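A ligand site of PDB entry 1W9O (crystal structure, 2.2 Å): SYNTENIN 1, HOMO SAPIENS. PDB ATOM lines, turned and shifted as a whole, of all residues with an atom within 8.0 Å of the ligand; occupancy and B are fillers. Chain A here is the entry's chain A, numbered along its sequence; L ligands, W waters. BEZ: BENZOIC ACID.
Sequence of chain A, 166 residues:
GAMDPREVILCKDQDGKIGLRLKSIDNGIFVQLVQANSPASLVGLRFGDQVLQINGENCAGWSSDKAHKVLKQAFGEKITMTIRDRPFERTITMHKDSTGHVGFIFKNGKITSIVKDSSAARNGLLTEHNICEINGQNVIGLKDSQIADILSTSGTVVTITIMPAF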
ATOM      1  N   ILE A  92      22.758  30.887 -14.188  1.00  0.00           N
ATOM      2  CA  ILE A  92      22.824  31.115 -15.625  1.00  0.00           C
ATOM      3  C   ILE A  92      21.765  30.298 -16.390  1.00  0.00           C
ATOM      4  O   ILE A  92      21.654  29.092 -16.219  1.00  0.00           O
ATOM      5  CB  ILE A  92      24.240  30.790 -16.165  1.00  0.00           C
ATOM      6  CG1 ILE A  92      25.260  31.799 -15.616  1.00  0.00           C
ATOM      7  CG2 ILE A  92      24.271  30.804 -17.709  1.00  0.00           C
ATOM      8  CD1 ILE A  92      24.979  33.251 -16.025  1.00  0.00           C
ATOM      9  N   THR A  93      21.006  31.002 -17.235  1.00  0.00           N
ATOM     10  CA  THR A  93      20.033  30.393 -18.115  1.00  0.00           C
ATOM     11  C   THR A  93      20.602  30.328 -19.531  1.00  0.00           C
ATOM     12  O   THR A  93      21.082  31.332 -20.072  1.00  0.00           O
ATOM     13  CB  THR A  93      18.724  31.208 -18.102  1.00  0.00           C
ATOM     14  OG1 THR A  93      18.207  31.303 -16.779  1.00  0.00           O
ATOM     15  CG2 THR A  93      17.635  30.465 -18.856  1.00  0.00           C
ATOM     16  N   MET A  94      20.523  29.145 -20.134  1.00  0.00           N
ATOM     17  CA  MET A  94      20.980  28.896 -21.496  1.00  0.00           C
ATOM     18  C   MET A  94      19.864  28.256 -22.335  1.00  0.00           C
ATOM     19  O   MET A  94      18.888  27.750 -21.791  1.00  0.00           O
ATOM     20  CB  MET A  94      22.216  28.020 -21.477  1.00  0.00           C
ATOM     21  CG  MET A  94      23.447  28.684 -20.868  1.00  0.00           C
ATOM     22  SD  MET A  94      24.700  27.520 -20.300  1.00  0.00           S
ATOM     23  CE  MET A  94      23.833  26.811 -18.888  1.00  0.00           C
ATOM     24  N   HIS A  95      20.022  28.315 -23.661  1.00  0.00           N
ATOM     25  CA  HIS A  95      19.100  27.709 -24.620  1.00  0.00           C
ATOM     26  C   HIS A  95      19.864  26.648 -25.407  1.00  0.00           C
ATOM     27  O   HIS A  95      20.933  26.917 -25.926  1.00  0.00           O
ATOM     28  CB  HIS A  95      18.534  28.749 -25.589  1.00  0.00           C
ATOM     29  CG  HIS A  95      17.421  29.584 -25.034  1.00  0.00           C
ATOM     30  ND1 HIS A  95      17.466  30.120 -23.771  1.00  0.00           N
ATOM     31  CD2 HIS A  95      16.245  29.972 -25.574  1.00  0.00           C
ATOM     32  CE1 HIS A  95      16.357  30.805 -23.545  1.00  0.00           C
ATOM     33  NE2 HIS A  95      15.596  30.722 -24.620  1.00  0.00           N
ATOM     34  N   LYS A  96      19.338  25.428 -25.474  1.00  0.00           N
ATOM     35  CA  LYS A  96      19.926  24.408 -26.340  1.00  0.00           C
ATOM     36  C   LYS A  96      19.792  24.851 -27.807  1.00  0.00           C
ATOM     37  O   LYS A  96      18.794  25.440 -28.190  1.00  0.00           O
ATOM     38  CB  LYS A  96      19.228  23.063 -26.178  1.00  0.00           C
ATOM     39  CG  LYS A  96      19.474  22.329 -24.874  1.00  0.00           C
ATOM     40  CD  LYS A  96      18.571  21.109 -24.785  1.00  0.00           C
ATOM     41  CE  LYS A  96      18.755  20.306 -23.508  1.00  0.00           C
ATOM     42  NZ  LYS A  96      17.803  19.146 -23.413  1.00  0.00           N
ATOM     43  N   ASP A  97      20.797  24.559 -28.625  1.00  0.00           N
ATOM     44  CA  ASP A  97      20.745  24.928 -30.034  1.00  0.00           C
ATOM     45  C   ASP A  97      19.985  23.829 -30.808  1.00  0.00           C
ATOM     46  O   ASP A  97      19.123  23.151 -30.220  1.00  0.00           O
ATOM     47  CB  ASP A  97      22.145  25.215 -30.591  1.00  0.00           C
ATOM     48  CG  ASP A  97      23.090  24.055 -30.482  1.00  0.00           C
ATOM     49  OD1 ASP A  97      22.634  22.900 -30.420  1.00  0.00           O
ATOM     50  OD2 ASP A  97      24.323  24.208 -30.460  1.00  0.00           O
ATOM     51  N   VAL A 102      23.734  23.101 -25.030  1.00  0.00           N
ATOM     52  CA  VAL A 102      23.873  24.483 -24.519  1.00  0.00           C
ATOM     53  C   VAL A 102      25.271  25.050 -24.734  1.00  0.00           C
ATOM     54  O   VAL A 102      25.435  26.242 -24.909  1.00  0.00           O
ATOM     55  CB  VAL A 102      23.528  24.611 -23.017  1.00  0.00           C
ATOM     56  CG1 VAL A 102      22.087  24.212 -22.762  1.00  0.00           C
ATOM     57  CG2 VAL A 102      24.501  23.807 -22.117  1.00  0.00           C
ATOM     58  N   ASP A 117      30.762  30.247 -29.432  1.00  0.00           N
ATOM     59  CA  ASP A 117      29.539  30.826 -29.952  1.00  0.00           C
ATOM     60  C   ASP A 117      28.247  30.056 -29.645  1.00  0.00           C
ATOM     61  O   ASP A 117      27.234  30.231 -30.303  1.00  0.00           O
ATOM     62  CB  ASP A 117      29.700  31.097 -31.455  1.00  0.00           C
ATOM     63  CG  ASP A 117      30.943  31.936 -31.761  1.00  0.00           C
ATOM     64  OD1 ASP A 117      31.372  32.713 -30.862  1.00  0.00           O
ATOM     65  OD2 ASP A 117      31.559  31.866 -32.861  1.00  0.00           O
ATOM     66  N   SER A 118      28.291  29.225 -28.599  1.00  0.00           N
ATOM     67  CA  SER A 118      27.096  28.556 -28.053  1.00  0.00           C
ATOM     68  C   SER A 118      26.350  29.479 -27.075  1.00  0.00           C
ATOM     69  O   SER A 118      26.796  30.598 -26.818  1.00  0.00           O
ATOM     70  CB  SER A 118      27.513  27.274 -27.334  1.00  0.00           C
ATOM     71  OG  SER A 118      28.440  27.544 -26.262  1.00  0.00           O
ATOM     72  N   SER A 119      25.200  29.041 -26.559  1.00  0.00           N
ATOM     73  CA  SER A 119      24.443  29.810 -25.575  1.00  0.00           C
ATOM     74  C   SER A 119      25.223  29.982 -24.265  1.00  0.00           C
ATOM     75  O   SER A 119      25.156  31.044 -23.641  1.00  0.00           O
ATOM     76  CB  SER A 119      23.095  29.165 -25.290  1.00  0.00           C
ATOM     77  OG  SER A 119      22.376  29.865 -24.286  1.00  0.00           O
ATOM     78  N   ALA A 120      25.971  28.947 -23.860  1.00  0.00           N
ATOM     79  CA  ALA A 120      26.892  29.073 -22.737  1.00  0.00           C
ATOM     80  C   ALA A 120      27.940  30.164 -22.961  1.00  0.00           C
ATOM     81  O   ALA A 120      28.331  30.844 -22.011  1.00  0.00           O
ATOM     82  CB  ALA A 120      27.576  27.726 -22.436  1.00  0.00           C
ATOM     83  N   ALA A 121      28.414  30.306 -24.199  1.00  0.00           N
ATOM     84  CA  ALA A 121      29.331  31.400 -24.529  1.00  0.00           C
ATOM     85  C   ALA A 121      28.658  32.760 -24.483  1.00  0.00           C
ATOM     86  O   ALA A 121      29.196  33.688 -23.874  1.00  0.00           O
ATOM     87  CB  ALA A 121      29.971  31.194 -25.887  1.00  0.00           C
ATOM     88  N   ARG A 122      27.499  32.884 -25.116  1.00  0.00           N
ATOM     89  CA  ARG A 122      26.749  34.138 -25.147  1.00  0.00           C
ATOM     90  C   ARG A 122      26.408  34.624 -23.736  1.00  0.00           C
ATOM     91  O   ARG A 122      26.409  35.852 -23.461  1.00  0.00           O
ATOM     92  CB  ARG A 122      25.447  33.989 -25.938  1.00  0.00           C
ATOM     93  CG  ARG A 122      25.649  33.933 -27.438  1.00  0.00           C
ATOM     94  CD  ARG A 122      24.385  34.089 -28.251  1.00  0.00           C
ATOM     95  NE  ARG A 122      23.495  32.947 -28.078  1.00  0.00           N
ATOM     96  CZ  ARG A 122      23.555  31.829 -28.788  1.00  0.00           C
ATOM     97  NH1 ARG A 122      24.459  31.665 -29.730  1.00  0.00           N
ATOM     98  NH2 ARG A 122      22.686  30.839 -28.559  1.00  0.00           N
ATOM     99  N   ASN A 123      26.139  33.661 -22.848  1.00  0.00           N
ATOM    100  CA  ASN A 123      25.724  33.931 -21.488  1.00  0.00           C
ATOM    101  C   ASN A 123      26.883  34.028 -20.498  1.00  0.00           C
ATOM    102  O   ASN A 123      26.662  34.152 -19.300  1.00  0.00           O
ATOM    103  CB  ASN A 123      24.750  32.855 -21.018  1.00  0.00           C
ATOM    104  CG  ASN A 123      23.321  33.124 -21.472  1.00  0.00           C
ATOM    105  OD1 ASN A 123      22.555  33.760 -20.763  1.00  0.00           O
ATOM    106  ND2 ASN A 123      22.970  32.613 -22.657  1.00  0.00           N
ATOM    107  N   THR A 156      14.276  22.962 -23.736  1.00  0.00           N
ATOM    108  CA  THR A 156      15.190  23.936 -24.338  1.00  0.00           C
ATOM    109  C   THR A 156      15.888  24.841 -23.313  1.00  0.00           C
ATOM    110  O   THR A 156      17.112  24.945 -23.300  1.00  0.00           O
ATOM    111  CB  THR A 156      14.414  24.759 -25.365  1.00  0.00           C
ATOM    112  OG1 THR A 156      14.090  23.920 -26.485  1.00  0.00           O
ATOM    113  CG2 THR A 156      15.282  25.900 -25.952  1.00  0.00           C
ATOM    114  N   VAL A 157      15.111  25.485 -22.439  1.00  0.00           N
ATOM    115  CA  VAL A 157      15.664  26.348 -21.393  1.00  0.00           C
ATOM    116  C   VAL A 157      16.331  25.515 -20.281  1.00  0.00           C
ATOM    117  O   VAL A 157      15.693  24.709 -19.604  1.00  0.00           O
ATOM    118  CB  VAL A 157      14.615  27.279 -20.759  1.00  0.00           C
ATOM    119  CG1 VAL A 157      15.310  28.349 -19.936  1.00  0.00           C
ATOM    120  CG2 VAL A 157      13.732  27.940 -21.840  1.00  0.00           C
ATOM    121  N   VAL A 158      17.635  25.717 -20.121  1.00  0.00           N
ATOM    122  CA  VAL A 158      18.422  25.048 -19.100  1.00  0.00           C
ATOM    123  C   VAL A 158      18.970  26.108 -18.150  1.00  0.00           C
ATOM    124  O   VAL A 158      19.784  26.940 -18.554  1.00  0.00           O
ATOM    125  CB  VAL A 158      19.580  24.247 -19.718  1.00  0.00           C
ATOM    126  CG1 VAL A 158      20.495  23.703 -18.627  1.00  0.00           C
ATOM    127  CG2 VAL A 158      19.037  23.111 -20.553  1.00  0.00           C
HETATM  128  C   BEZ L   1      20.409  32.115 -25.269  1.00  0.00           C
HETATM  129  O1  BEZ L   1      20.490  32.390 -23.900  1.00  0.00           O
HETATM  130  O2  BEZ L   1      21.440  31.570 -25.857  1.00  0.00           O
HETATM  131  C1  BEZ L   1      19.172  32.402 -26.047  1.00  0.00           C
HETATM  132  C2  BEZ L   1      18.993  31.814 -27.306  1.00  0.00           C
HETATM  133  C3  BEZ L   1      17.825  32.046 -28.014  1.00  0.00           C
HETATM  134  C4  BEZ L   1      16.841  32.876 -27.484  1.00  0.00           C
HETATM  135  C5  BEZ L   1      17.020  33.472 -26.229  1.00  0.00           C
HETATM  136  C6  BEZ L   1      18.187  33.223 -25.512  1.00  0.00           C
HETATM  137  O   HOH W   1      19.215  32.554 -21.786  1.00  0.00           O
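Merely in contact with the ligand: His 95 (3.5 Å). Of the 17 residues printed, 4 come within 4 Å of the ligand.
Water W1 lies within hydrogen-bond range of O1 of the ligand (2.5 Å) and O of Thr 93 (2.8 Å).
The backbone carbonyl oxygen (O) of Ser 119 is in hydrogen-bond range of the side-chain amide nitrogen (ND2) of Asn 123, at 2.9 Å. O of Val 102 lies within hydrogen-bond range of N of Ser 119, 3.3 Å away. The backbone carbonyl oxygen of Thr 93 sits close to the side-chain amide oxygen of Asn 123, 2.9 Å away. The guanidinium group of Arg 122 is in hydrogen-bond range of the backbone carbonyl oxygen of Asp 117, at 3.2 Å. The backbone NH (N) of His 95 lies within hydrogen-bond range of the side-chain hydroxyl (OG) of Ser 119 (2.9 Å).
The side-chain hydroxyl of Ser 119 lies within hydrogen-bond range of an oxygen (O2) of the ligand, at 2.5 Å. ND2 of Asn 123 lies within hydrogen-bond range of O1 of the ligand. O2 of the ligand lies within salt-bridge range of NH2 of Arg 122, at 3.1 Å.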
